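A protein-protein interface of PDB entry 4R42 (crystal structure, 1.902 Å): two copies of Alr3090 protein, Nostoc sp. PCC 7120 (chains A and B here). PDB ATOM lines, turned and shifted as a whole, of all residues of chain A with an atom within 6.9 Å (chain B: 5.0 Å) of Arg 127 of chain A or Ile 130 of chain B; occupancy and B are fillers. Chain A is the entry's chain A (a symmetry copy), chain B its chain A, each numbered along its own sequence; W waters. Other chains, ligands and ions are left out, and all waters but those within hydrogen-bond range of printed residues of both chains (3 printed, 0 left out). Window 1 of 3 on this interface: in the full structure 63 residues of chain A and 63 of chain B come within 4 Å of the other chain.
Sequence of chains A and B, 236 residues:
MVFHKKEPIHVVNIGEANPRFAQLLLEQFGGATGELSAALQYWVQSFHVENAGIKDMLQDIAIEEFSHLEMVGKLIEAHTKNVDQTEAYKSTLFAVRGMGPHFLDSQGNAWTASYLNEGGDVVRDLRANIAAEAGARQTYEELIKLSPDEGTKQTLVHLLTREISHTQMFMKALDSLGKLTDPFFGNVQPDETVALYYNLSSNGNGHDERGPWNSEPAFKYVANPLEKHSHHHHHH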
ATOM      1  N   GLN A  41      18.734 -36.088   8.658  1.00  0.00           N
ATOM      2  CA  GLN A  41      19.716 -35.054   8.368  1.00  0.00           C
ATOM      3  C   GLN A  41      20.139 -34.342   9.648  1.00  0.00           C
ATOM      4  O   GLN A  41      21.330 -34.202   9.926  1.00  0.00           O
ATOM      5  CB  GLN A  41      19.166 -34.043   7.368  1.00  0.00           C
ATOM      6  CG  GLN A  41      20.203 -33.017   6.953  1.00  0.00           C
ATOM      7  CD  GLN A  41      19.880 -32.366   5.639  1.00  0.00           C
ATOM      8  OE1 GLN A  41      19.763 -33.039   4.603  1.00  0.00           O
ATOM      9  NE2 GLN A  41      19.740 -31.051   5.661  1.00  0.00           N
ATOM     10  N   GLN A  45      23.780 -34.817  11.803  1.00  0.00           N
ATOM     11  CA  GLN A  45      24.623 -33.640  11.988  1.00  0.00           C
ATOM     12  C   GLN A  45      25.028 -33.477  13.444  1.00  0.00           C
ATOM     13  O   GLN A  45      26.148 -33.056  13.745  1.00  0.00           O
ATOM     14  CB  GLN A  45      23.914 -32.372  11.515  1.00  0.00           C
ATOM     15  CG  GLN A  45      23.773 -32.261  10.012  1.00  0.00           C
ATOM     16  CD  GLN A  45      22.739 -31.235   9.612  1.00  0.00           C
ATOM     17  OE1 GLN A  45      21.949 -30.763  10.441  1.00  0.00           O
ATOM     18  NE2 GLN A  45      22.739 -30.874   8.334  1.00  0.00           N
ATOM     19  N   ASN A 117      21.991 -33.585   2.850  1.00  0.00           N
ATOM     20  CA  ASN A 117      23.106 -32.659   2.675  1.00  0.00           C
ATOM     21  C   ASN A 117      23.675 -32.301   4.048  1.00  0.00           C
ATOM     22  O   ASN A 117      23.043 -31.585   4.806  1.00  0.00           O
ATOM     23  CB  ASN A 117      22.627 -31.421   1.925  1.00  0.00           C
ATOM     24  CG  ASN A 117      23.751 -30.439   1.595  1.00  0.00           C
ATOM     25  OD1 ASN A 117      24.882 -30.564   2.061  1.00  0.00           O
ATOM     26  ND2 ASN A 117      23.431 -29.454   0.773  1.00  0.00           N
ATOM     27  N   VAL A 122      29.298 -26.685  10.825  1.00  0.00           N
ATOM     28  CA  VAL A 122      27.935 -26.384  11.260  1.00  0.00           C
ATOM     29  C   VAL A 122      27.255 -25.345  10.367  1.00  0.00           C
ATOM     30  O   VAL A 122      26.024 -25.345  10.228  1.00  0.00           O
ATOM     31  CB  VAL A 122      27.924 -25.904  12.730  1.00  0.00           C
ATOM     32  CG1 VAL A 122      28.643 -24.561  12.904  1.00  0.00           C
ATOM     33  CG2 VAL A 122      26.504 -25.842  13.257  1.00  0.00           C
ATOM     34  N   VAL A 123      28.039 -24.472   9.741  1.00  0.00           N
ATOM     35  CA  VAL A 123      27.456 -23.469   8.852  1.00  0.00           C
ATOM     36  C   VAL A 123      26.896 -24.121   7.589  1.00  0.00           C
ATOM     37  O   VAL A 123      25.803 -23.767   7.134  1.00  0.00           O
ATOM     38  CB  VAL A 123      28.480 -22.375   8.471  1.00  0.00           C
ATOM     39  CG1 VAL A 123      27.906 -21.438   7.408  1.00  0.00           C
ATOM     40  CG2 VAL A 123      28.863 -21.555   9.701  1.00  0.00           C
ATOM     41  N   ARG A 124      27.638 -25.061   7.018  1.00  0.00           N
ATOM     42  CA  ARG A 124      27.126 -25.852   5.895  1.00  0.00           C
ATOM     43  C   ARG A 124      25.850 -26.607   6.302  1.00  0.00           C
ATOM     44  O   ARG A 124      24.850 -26.619   5.576  1.00  0.00           O
ATOM     45  CB  ARG A 124      28.203 -26.826   5.402  1.00  0.00           C
ATOM     46  CG  ARG A 124      27.730 -27.796   4.310  1.00  0.00           C
ATOM     47  CD  ARG A 124      27.187 -29.119   4.870  1.00  0.00           C
ATOM     48  NE  ARG A 124      26.960 -30.069   3.778  1.00  0.00           N
ATOM     49  CZ  ARG A 124      27.899 -30.829   3.232  1.00  0.00           C
ATOM     50  NH1 ARG A 124      27.592 -31.620   2.214  1.00  0.00           N
ATOM     51  NH2 ARG A 124      29.138 -30.811   3.700  1.00  0.00           N
ATOM     52  N   ASP A 125      25.883 -27.227   7.472  1.00  0.00           N
ATOM     53  CA  ASP A 125      24.739 -27.995   7.962  1.00  0.00           C
ATOM     54  C   ASP A 125      23.503 -27.126   8.103  1.00  0.00           C
ATOM     55  O   ASP A 125      22.438 -27.464   7.592  1.00  0.00           O
ATOM     56  CB  ASP A 125      25.072 -28.647   9.300  1.00  0.00           C
ATOM     57  CG  ASP A 125      26.073 -29.779   9.171  1.00  0.00           C
ATOM     58  OD1 ASP A 125      26.146 -30.419   8.095  1.00  0.00           O
ATOM     59  OD2 ASP A 125      26.762 -30.052  10.178  1.00  0.00           O
ATOM     60  N   LEU A 126      23.641 -25.981   8.753  1.00  0.00           N
ATOM     61  CA  LEU A 126      22.481 -25.113   8.953  1.00  0.00           C
ATOM     62  C   LEU A 126      21.931 -24.571   7.641  1.00  0.00           C
ATOM     63  O   LEU A 126      20.718 -24.469   7.477  1.00  0.00           O
ATOM     64  CB  LEU A 126      22.836 -23.961   9.875  1.00  0.00           C
ATOM     65  CG  LEU A 126      23.097 -24.391  11.321  1.00  0.00           C
ATOM     66  CD1 LEU A 126      23.676 -23.237  12.136  1.00  0.00           C
ATOM     67  CD2 LEU A 126      21.832 -24.899  11.980  1.00  0.00           C
ATOM     68  N   ARG A 127      22.813 -24.228   6.708  1.00  0.00           N
ATOM     69  CA  ARG A 127      22.356 -23.748   5.403  1.00  0.00           C
ATOM     70  C   ARG A 127      21.625 -24.869   4.685  1.00  0.00           C
ATOM     71  O   ARG A 127      20.577 -24.642   4.066  1.00  0.00           O
ATOM     72  CB  ARG A 127      23.526 -23.218   4.571  1.00  0.00           C
ATOM     73  CG  ARG A 127      23.980 -21.847   5.049  1.00  0.00           C
ATOM     74  CD  ARG A 127      25.149 -21.271   4.250  1.00  0.00           C
ATOM     75  NE  ARG A 127      25.571 -20.001   4.859  1.00  0.00           N
ATOM     76  CZ  ARG A 127      26.634 -19.291   4.496  1.00  0.00           C
ATOM     77  NH1 ARG A 127      27.398 -19.682   3.487  1.00  0.00           N
ATOM     78  NH2 ARG A 127      26.920 -18.157   5.137  1.00  0.00           N
ATOM     79  N   ALA A 128      22.169 -26.080   4.784  1.00  0.00           N
ATOM     80  CA  ALA A 128      21.500 -27.267   4.244  1.00  0.00           C
ATOM     81  C   ALA A 128      20.120 -27.475   4.875  1.00  0.00           C
ATOM     82  O   ALA A 128      19.176 -27.904   4.203  1.00  0.00           O
ATOM     83  CB  ALA A 128      22.362 -28.508   4.449  1.00  0.00           C
ATOM     84  N   ASN A 129      19.991 -27.182   6.161  1.00  0.00           N
ATOM     85  CA  ASN A 129      18.727 -27.423   6.838  1.00  0.00           C
ATOM     86  C   ASN A 129      17.669 -26.403   6.428  1.00  0.00           C
ATOM     87  O   ASN A 129      16.489 -26.738   6.262  1.00  0.00           O
ATOM     88  CB  ASN A 129      18.940 -27.438   8.357  1.00  0.00           C
ATOM     89  CG  ASN A 129      19.851 -28.574   8.788  1.00  0.00           C
ATOM     90  OD1 ASN A 129      20.144 -29.474   7.998  1.00  0.00           O
ATOM     91  ND2 ASN A 129      20.325 -28.524  10.020  1.00  0.00           N
ATOM     92  N   ILE A 130      18.087 -25.164   6.218  1.00  0.00           N
ATOM     93  CA  ILE A 130      17.160 -24.151   5.726  1.00  0.00           C
ATOM     94  C   ILE A 130      16.641 -24.566   4.345  1.00  0.00           C
ATOM     95  O   ILE A 130      15.464 -24.394   4.045  1.00  0.00           O
ATOM     96  CB  ILE A 130      17.823 -22.759   5.681  1.00  0.00           C
ATOM     97  CG1 ILE A 130      17.945 -22.206   7.107  1.00  0.00           C
ATOM     98  CG2 ILE A 130      16.995 -21.793   4.840  1.00  0.00           C
ATOM     99  CD1 ILE A 130      18.852 -21.019   7.234  1.00  0.00           C
ATOM    100  N   ALA A 131      17.506 -25.161   3.528  1.00  0.00           N
ATOM    101  CA  ALA A 131      17.101 -25.682   2.221  1.00  0.00           C
ATOM    102  C   ALA A 131      16.138 -26.855   2.347  1.00  0.00           C
ATOM    103  O   ALA A 131      15.175 -26.967   1.585  1.00  0.00           O
ATOM    104  CB  ALA A 131      18.329 -26.123   1.412  1.00  0.00           C
ATOM    105  N   ALA A 132      16.422 -27.750   3.291  1.00  0.00           N
ATOM    106  CA  ALA A 132      15.600 -28.929   3.492  1.00  0.00           C
ATOM    107  C   ALA A 132      14.198 -28.483   3.879  1.00  0.00           C
ATOM    108  O   ALA A 132      13.203 -28.951   3.303  1.00  0.00           O
ATOM    109  CB  ALA A 132      16.200 -29.837   4.559  1.00  0.00           C
ATOM    110  N   PHE A 170      16.511 -22.466  12.535  1.00  0.00           N
ATOM    111  CA  PHE A 170      17.786 -22.543  11.816  1.00  0.00           C
ATOM    112  C   PHE A 170      18.340 -21.167  11.441  1.00  0.00           C
ATOM    113  O   PHE A 170      19.561 -20.934  11.473  1.00  0.00           O
ATOM    114  CB  PHE A 170      17.626 -23.409  10.558  1.00  0.00           C
ATOM    115  CG  PHE A 170      17.373 -24.869  10.862  1.00  0.00           C
ATOM    116  CD1 PHE A 170      18.225 -25.570  11.694  1.00  0.00           C
ATOM    117  CD2 PHE A 170      16.278 -25.525  10.336  1.00  0.00           C
ATOM    118  CE1 PHE A 170      18.001 -26.906  11.980  1.00  0.00           C
ATOM    119  CE2 PHE A 170      16.049 -26.860  10.624  1.00  0.00           C
ATOM    120  CZ  PHE A 170      16.907 -27.544  11.446  1.00  0.00           C
ATOM    121  N   LEU A 174      21.969 -19.694  12.670  1.00  0.00           N
ATOM    122  CA  LEU A 174      22.972 -19.191  11.723  1.00  0.00           C
ATOM    123  C   LEU A 174      23.347 -17.760  12.024  1.00  0.00           C
ATOM    124  O   LEU A 174      24.510 -17.368  11.908  1.00  0.00           O
ATOM    125  CB  LEU A 174      22.459 -19.261  10.293  1.00  0.00           C
ATOM    126  CG  LEU A 174      22.901 -20.422   9.428  1.00  0.00           C
ATOM    127  CD1 LEU A 174      22.174 -20.324   8.104  1.00  0.00           C
ATOM    128  CD2 LEU A 174      24.415 -20.441   9.218  1.00  0.00           C
ATOM    129  N   GLY A 178      26.785 -15.326  12.994  1.00  0.00           N
ATOM    130  CA  GLY A 178      27.104 -14.273  12.039  1.00  0.00           C
ATOM    131  C   GLY A 178      27.109 -14.733  10.590  1.00  0.00           C
ATOM    132  O   GLY A 178      27.711 -14.080   9.734  1.00  0.00           O
ATOM    133  N   LYS A 179      26.416 -15.834  10.294  1.00  0.00           N
ATOM    134  CA  LYS A 179      26.516 -16.468   8.983  1.00  0.00           C
ATOM    135  C   LYS A 179      25.183 -16.639   8.257  1.00  0.00           C
ATOM    136  O   LYS A 179      25.091 -17.404   7.298  1.00  0.00           O
ATOM    137  CB  LYS A 179      27.210 -17.836   9.120  1.00  0.00           C
ATOM    138  CG  LYS A 179      28.657 -17.750   9.612  1.00  0.00           C
ATOM    139  CD  LYS A 179      29.508 -16.908   8.677  1.00  0.00           C
ATOM    140  CE  LYS A 179      30.912 -16.663   9.188  1.00  0.00           C
ATOM    141  NZ  LYS A 179      31.603 -15.665   8.291  1.00  0.00           N
ATOM    142  N   LEU A 180      24.160 -15.911   8.680  1.00  0.00           N
ATOM    143  CA  LEU A 180      22.895 -15.931   7.952  1.00  0.00           C
ATOM    144  C   LEU A 180      22.983 -15.030   6.702  1.00  0.00           C
ATOM    145  O   LEU A 180      22.512 -15.408   5.623  1.00  0.00           O
ATOM    146  CB  LEU A 180      21.746 -15.507   8.872  1.00  0.00           C
ATOM    147  CG  LEU A 180      20.341 -15.444   8.252  1.00  0.00           C
ATOM    148  CD1 LEU A 180      19.898 -16.790   7.738  1.00  0.00           C
ATOM    149  CD2 LEU A 180      19.345 -14.905   9.244  1.00  0.00           C
ATOM    150  N   THR A 181      23.623 -13.872   6.845  1.00  0.00           N
ATOM    151  CA  THR A 181      23.703 -12.883   5.767  1.00  0.00           C
ATOM    152  C   THR A 181      25.127 -12.617   5.260  1.00  0.00           C
ATOM    153  O   THR A 181      25.321 -11.765   4.397  1.00  0.00           O
ATOM    154  CB  THR A 181      23.104 -11.543   6.213  1.00  0.00           C
ATOM    155  OG1 THR A 181      23.844 -11.029   7.326  1.00  0.00           O
ATOM    156  CG2 THR A 181      21.657 -11.730   6.619  1.00  0.00           C
ATOM    157  N   ASP A 182      26.103 -13.338   5.803  1.00  0.00           N
ATOM    158  CA  ASP A 182      27.497 -13.264   5.361  1.00  0.00           C
ATOM    159  C   ASP A 182      27.839 -14.535   4.591  1.00  0.00           C
ATOM    160  O   ASP A 182      27.734 -15.624   5.144  1.00  0.00           O
ATOM    161  CB  ASP A 182      28.420 -13.095   6.577  1.00  0.00           C
ATOM    162  CG  ASP A 182      29.886 -12.921   6.200  1.00  0.00           C
ATOM    163  OD1 ASP A 182      30.291 -13.244   5.064  1.00  0.00           O
ATOM    164  OD2 ASP A 182      30.643 -12.467   7.074  1.00  0.00           O
ATOM    165  N   PRO A 183      28.265 -14.408   3.317  1.00  0.00           N
ATOM    166  CA  PRO A 183      28.484 -15.613   2.514  1.00  0.00           C
ATOM    167  C   PRO A 183      29.657 -16.458   2.993  1.00  0.00           C
ATOM    168  O   PRO A 183      29.651 -17.673   2.815  1.00  0.00           O
ATOM    169  CB  PRO A 183      28.764 -15.049   1.112  1.00  0.00           C
ATOM    170  CG  PRO A 183      29.316 -13.724   1.358  1.00  0.00           C
ATOM    171  CD  PRO A 183      28.549 -13.191   2.533  1.00  0.00           C
ATOM    172  N   PHE A 184      30.641 -15.814   3.608  1.00  0.00           N
ATOM    173  CA  PHE A 184      31.906 -16.463   3.901  1.00  0.00           C
ATOM    174  C   PHE A 184      31.833 -17.370   5.123  1.00  0.00           C
ATOM    175  O   PHE A 184      31.305 -16.988   6.162  1.00  0.00           O
ATOM    176  CB  PHE A 184      33.009 -15.420   4.110  1.00  0.00           C
ATOM    177  CG  PHE A 184      34.340 -16.035   4.424  1.00  0.00           C
ATOM    178  CD1 PHE A 184      35.129 -16.555   3.414  1.00  0.00           C
ATOM    179  CD2 PHE A 184      34.772 -16.152   5.730  1.00  0.00           C
ATOM    180  CE1 PHE A 184      36.331 -17.149   3.692  1.00  0.00           C
ATOM    181  CE2 PHE A 184      35.980 -16.749   6.023  1.00  0.00           C
ATOM    182  CZ  PHE A 184      36.766 -17.250   5.004  1.00  0.00           C
ATOM    183  N   PHE A 185      32.376 -18.576   4.988  1.00  0.00           N
ATOM    184  CA  PHE A 185      32.658 -19.407   6.156  1.00  0.00           C
ATOM    185  C   PHE A 185      33.825 -20.313   5.843  1.00  0.00           C
ATOM    186  O   PHE A 185      34.388 -20.254   4.740  1.00  0.00           O
ATOM    187  CB  PHE A 185      31.420 -20.207   6.607  1.00  0.00           C
ATOM    188  CG  PHE A 185      31.037 -21.375   5.712  1.00  0.00           C
ATOM    189  CD1 PHE A 185      30.403 -21.168   4.500  1.00  0.00           C
ATOM    190  CD2 PHE A 185      31.259 -22.689   6.126  1.00  0.00           C
ATOM    191  CE1 PHE A 185      30.036 -22.243   3.693  1.00  0.00           C
ATOM    192  CE2 PHE A 185      30.883 -23.763   5.329  1.00  0.00           C
ATOM    193  CZ  PHE A 185      30.269 -23.543   4.121  1.00  0.00           C
ATOM    194  N   LEU B 126      16.439 -20.832  -4.338  1.00  0.00           N
ATOM    195  CA  LEU B 126      17.583 -20.044  -3.877  1.00  0.00           C
ATOM    196  C   LEU B 126      18.133 -20.545  -2.549  1.00  0.00           C
ATOM    197  O   LEU B 126      19.345 -20.563  -2.351  1.00  0.00           O
ATOM    198  CB  LEU B 126      17.202 -18.580  -3.756  1.00  0.00           C
ATOM    199  CG  LEU B 126      16.939 -17.901  -5.103  1.00  0.00           C
ATOM    200  CD1 LEU B 126      16.335 -16.514  -4.905  1.00  0.00           C
ATOM    201  CD2 LEU B 126      18.208 -17.795  -5.923  1.00  0.00           C
ATOM    202  N   ARG B 127      17.252 -20.953  -1.642  1.00  0.00           N
ATOM    203  CA  ARG B 127      17.709 -21.495  -0.362  1.00  0.00           C
ATOM    204  C   ARG B 127      18.463 -22.790  -0.607  1.00  0.00           C
ATOM    205  O   ARG B 127      19.513 -23.033   0.006  1.00  0.00           O
ATOM    206  CB  ARG B 127      16.536 -21.703   0.599  1.00  0.00           C
ATOM    207  CG  ARG B 127      16.055 -20.387   1.192  1.00  0.00           C
ATOM    208  CD  ARG B 127      14.882 -20.539   2.160  1.00  0.00           C
ATOM    209  NE  ARG B 127      14.434 -19.205   2.590  1.00  0.00           N
ATOM    210  CZ  ARG B 127      13.362 -18.958   3.335  1.00  0.00           C
ATOM    211  NH1 ARG B 127      12.612 -19.950   3.792  1.00  0.00           N
ATOM    212  NH2 ARG B 127      13.052 -17.700   3.648  1.00  0.00           N
ATOM    213  N   ALA B 128      17.940 -23.610  -1.516  1.00  0.00           N
ATOM    214  CA  ALA B 128      18.633 -24.830  -1.936  1.00  0.00           C
ATOM    215  C   ALA B 128      20.012 -24.524  -2.528  1.00  0.00           C
ATOM    216  O   ALA B 128      20.967 -25.281  -2.329  1.00  0.00           O
ATOM    217  CB  ALA B 128      17.790 -25.604  -2.945  1.00  0.00           C
ATOM    218  N   ASN B 129      20.127 -23.424  -3.259  1.00  0.00           N
ATOM    219  CA  ASN B 129      21.390 -23.112  -3.907  1.00  0.00           C
ATOM    220  C   ASN B 129      22.434 -22.636  -2.900  1.00  0.00           C
ATOM    221  O   ASN B 129      23.620 -22.973  -3.002  1.00  0.00           O
ATOM    222  CB  ASN B 129      21.167 -22.081  -5.021  1.00  0.00           C
ATOM    223  CG  ASN B 129      20.273 -22.624  -6.121  1.00  0.00           C
ATOM    224  OD1 ASN B 129      20.001 -23.825  -6.169  1.00  0.00           O
ATOM    225  ND2 ASN B 129      19.790 -21.748  -6.984  1.00  0.00           N
ATOM    226  N   ILE B 130      21.996 -21.889  -1.898  1.00  0.00           N
ATOM    227  CA  ILE B 130      22.909 -21.476  -0.838  1.00  0.00           C
ATOM    228  C   ILE B 130      23.444 -22.719  -0.118  1.00  0.00           C
ATOM    229  O   ILE B 130      24.620 -22.780   0.226  1.00  0.00           O
ATOM    230  CB  ILE B 130      22.223 -20.510   0.148  1.00  0.00           C
ATOM    231  CG1 ILE B 130      22.081 -19.129  -0.507  1.00  0.00           C
ATOM    232  CG2 ILE B 130      23.040 -20.373   1.428  1.00  0.00           C
ATOM    233  CD1 ILE B 130      21.154 -18.195   0.212  1.00  0.00           C
ATOM    234  N   ALA B 131      22.595 -23.728   0.060  1.00  0.00           N
ATOM    235  CA  ALA B 131      23.018 -24.998   0.652  1.00  0.00           C
ATOM    236  C   ALA B 131      23.999 -25.746  -0.240  1.00  0.00           C
ATOM    237  O   ALA B 131      24.969 -26.336   0.243  1.00  0.00           O
ATOM    238  CB  ALA B 131      21.802 -25.895   0.927  1.00  0.00           C
ATOM    239  N   ALA B 132      23.725 -25.750  -1.543  1.00  0.00           N
ATOM    240  CA  ALA B 132      24.565 -26.454  -2.494  1.00  0.00           C
ATOM    241  C   ALA B 132      25.956 -25.840  -2.458  1.00  0.00           C
ATOM    242  O   ALA B 132      26.963 -26.559  -2.356  1.00  0.00           O
ATOM    243  CB  ALA B 132      23.973 -26.388  -3.897  1.00  0.00           C
ATOM    244  N   GLU B 133      26.005 -24.511  -2.525  1.00  0.00           N
ATOM    245  CA  GLU B 133      27.269 -23.785  -2.471  1.00  0.00           C
ATOM    246  C   GLU B 133      28.020 -24.094  -1.183  1.00  0.00           C
ATOM    247  O   GLU B 133      29.246 -24.121  -1.177  1.00  0.00           O
ATOM    248  CB  GLU B 133      27.045 -22.271  -2.578  1.00  0.00           C
ATOM    249  CG  GLU B 133      26.472 -21.799  -3.914  1.00  0.00           C
ATOM    250  CD  GLU B 133      27.429 -21.963  -5.074  1.00  0.00           C
ATOM    251  OE1 GLU B 133      28.651 -21.886  -4.850  1.00  0.00           O
ATOM    252  OE2 GLU B 133      26.953 -22.167  -6.219  1.00  0.00           O
ATOM    253  N   ALA B 134      27.300 -24.278  -0.078  1.00  0.00           N
ATOM    254  CA  ALA B 134      27.977 -24.533   1.187  1.00  0.00           C
ATOM    255  C   ALA B 134      28.646 -25.913   1.153  1.00  0.00           C
ATOM    256  O   ALA B 134      29.768 -26.085   1.629  1.00  0.00           O
ATOM    257  CB  ALA B 134      27.007 -24.432   2.352  1.00  0.00           C
ATOM    258  N   THR B 167      27.614 -17.799  -3.468  1.00  0.00           N
ATOM    259  CA  THR B 167      26.801 -17.718  -2.250  1.00  0.00           C
ATOM    260  C   THR B 167      26.283 -16.292  -2.073  1.00  0.00           C
ATOM    261  O   THR B 167      25.115 -16.067  -1.761  1.00  0.00           O
ATOM    262  CB  THR B 167      27.595 -18.130  -0.989  1.00  0.00           C
ATOM    263  OG1 THR B 167      28.022 -19.490  -1.125  1.00  0.00           O
ATOM    264  CG2 THR B 167      26.732 -17.985   0.275  1.00  0.00           C
ATOM    265  N   PHE B 170      23.483 -15.558  -4.614  1.00  0.00           N
ATOM    266  CA  PHE B 170      22.214 -16.130  -4.155  1.00  0.00           C
ATOM    267  C   PHE B 170      21.640 -15.400  -2.940  1.00  0.00           C
ATOM    268  O   PHE B 170      20.415 -15.229  -2.811  1.00  0.00           O
ATOM    269  CB  PHE B 170      22.398 -17.622  -3.837  1.00  0.00           C
ATOM    270  CG  PHE B 170      22.673 -18.467  -5.060  1.00  0.00           C
ATOM    271  CD1 PHE B 170      21.828 -18.418  -6.152  1.00  0.00           C
ATOM    272  CD2 PHE B 170      23.783 -19.287  -5.122  1.00  0.00           C
ATOM    273  CE1 PHE B 170      22.073 -19.187  -7.278  1.00  0.00           C
ATOM    274  CE2 PHE B 170      24.032 -20.053  -6.248  1.00  0.00           C
ATOM    275  CZ  PHE B 170      23.181 -19.998  -7.321  1.00  0.00           C
ATOM    276  N   MET B 171      22.499 -14.968  -2.027  1.00  0.00           N
ATOM    277  CA  MET B 171      21.994 -14.218  -0.882  1.00  0.00           C
ATOM    278  C   MET B 171      21.398 -12.878  -1.333  1.00  0.00           C
ATOM    279  O   MET B 171      20.357 -12.467  -0.831  1.00  0.00           O
ATOM    280  CB  MET B 171      23.088 -13.990   0.148  1.00  0.00           C
ATOM    281  CG  MET B 171      23.439 -15.214   0.968  1.00  0.00           C
ATOM    282  SD  MET B 171      24.764 -14.812   2.132  1.00  0.00           S
ATOM    283  CE  MET B 171      24.803 -16.304   3.109  1.00  0.00           C
ATOM    284  N   LEU B 174      17.978 -13.547  -2.842  1.00  0.00           N
ATOM    285  CA  LEU B 174      16.973 -13.851  -1.816  1.00  0.00           C
ATOM    286  C   LEU B 174      16.572 -12.612  -1.052  1.00  0.00           C
ATOM    287  O   LEU B 174      15.403 -12.427  -0.706  1.00  0.00           O
ATOM    288  CB  LEU B 174      17.497 -14.877  -0.823  1.00  0.00           C
ATOM    289  CG  LEU B 174      17.081 -16.321  -0.997  1.00  0.00           C
ATOM    290  CD1 LEU B 174      17.814 -17.150   0.036  1.00  0.00           C
ATOM    291  CD2 LEU B 174      15.568 -16.506  -0.868  1.00  0.00           C
ATOM    292  N   LEU B 180      15.750 -13.585   2.641  1.00  0.00           N
ATOM    293  CA  LEU B 180      17.021 -14.079   3.164  1.00  0.00           C
ATOM    294  C   LEU B 180      16.925 -14.287   4.690  1.00  0.00           C
ATOM    295  O   LEU B 180      17.410 -15.296   5.217  1.00  0.00           O
ATOM    296  CB  LEU B 180      18.155 -13.120   2.796  1.00  0.00           C
ATOM    297  CG  LEU B 180      19.563 -13.476   3.299  1.00  0.00           C
ATOM    298  CD1 LEU B 180      20.032 -14.799   2.749  1.00  0.00           C
ATOM    299  CD2 LEU B 180      20.543 -12.386   2.956  1.00  0.00           C
HETATM  300  O   HOH W   1      13.188 -22.643   4.484  1.00  0.00           O
HETATM  301  O   HOH W   2      20.030 -22.324   2.639  1.00  0.00           O
HETATM  302  O   HOH W   3      26.863 -21.170   1.128  1.00  0.00           O
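The backbone nitrogen (N) of Pro 183 of chain A lies close to the side-chain sulfur (SD) of Met 171 of chain B.
OE1 of Gln 41 of chain A lies within hydrogen-bond range of N of Asn 117 of chain A, at 2.9 Å. The backbone carbonyl oxygen of Asp 182 of chain A lies within hydrogen-bond range of the guanidinium group of Arg 127 of chain A (2.7 Å). The side-chain amino group of Lys 179 of chain A is in salt-bridge range of the side-chain carboxylate of Asp 182 of chain A, 3.6 Å away.
Among the printed residues, pairs that only touch across the chains: Arg 127 of chain A with Met 171 of chain B, Ala 131 of chain A with Ala 131 of chain B, Asn 117 of chain A with Ala 131 of chain B, Leu 180 of chain A with Met 171 of chain B, Phe 185 of chain A with Ala 134 of chain B, Arg 127 of chain A with Ala 131 of chain B, Ala 131 of chain A with Arg 127 of chain B, Ala 131 of chain A with Ala 128 of chain B, Ala 128 of chain A with Ala 131 of chain B, Asp 182 of chain A with Met 171 of chain B, Arg 127 of chain A with Ile 130 of chain B, Ile 130 of chain A with Arg 127 of chain B, Pro 183 of chain A with Thr 167 of chain B, Arg 127 of chain A with Thr 167 of chain B, Arg 124 of chain A with Ala 134 of chain B, Thr 181 of chain A with Met 171 of chain B, Leu 180 of chain A with Leu 180 of chain B and Thr 181 of chain A with Leu 180 of chain B.
Of the printed residues of chain B, Arg 124 of chain A touches Ala 134 (3.8 Å). Phe 170 of chain A touches none of the printed residues of chain B. Printed residues of chain A within 4 Å of Arg 127 of chain B: Ile 130 and Ala 131. Of chain A, only Arg 127 comes within 4 Å of Ile 130 of chain B. Of the printed residues of chain A, Thr 167 of chain B touches Arg 127 (3.7 Å) and Pro 183 (3.7 Å). The nearest residue of chain A that does not touch Ile 130 of chain B is Ala 128 of chain A (6.1 Å). The nearest printed residue of chain A that does not touch Leu 180 of chain B is Ile 130 of chain A (6.2 Å).
Hydrophobic or aromatic side chains of chain B that line the printed part of chain A: Ile 130, Ala 131, Ala 134, Met 171 and Leu 180. Printed residues of chain A that touch a printed residue of chain B: Asn 117, Arg 124, Arg 127, Ala 128, Ile 130, Ala 131, Leu 180, Thr 181, Asp 182, Pro 183 and Phe 185. Among the printed residues, 19 pairs touch across the chains. Among the printed residues, no Asp or Glu carboxylate lies within 4 Å of a Lys or Arg side-chain nitrogen of the other chain.
Arg 127 of chain A touches Ile 130 of chain B, and with the chains exchanged Ile 130 of chain A touches Arg 127 of chain B. Arg 127 of chain A touches Ala 131 of chain B, and with the chains exchanged Ala 131 of chain A touches Arg 127 of chain B. Leu 180 of chain B touches its own counterpart, Leu 180 of chain A.
Water W2 lies within hydrogen-bond range of O of Arg 127 of chain B (2.8 Å) and O of Arg 127 of chain A (2.8 Å). Water W3 lies within hydrogen-bond range of NH1 of Arg 127 of chain A, O of Ile 130 of chain B, OG1 of Thr 167 of chain B and N of Ala 134 of chain B.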
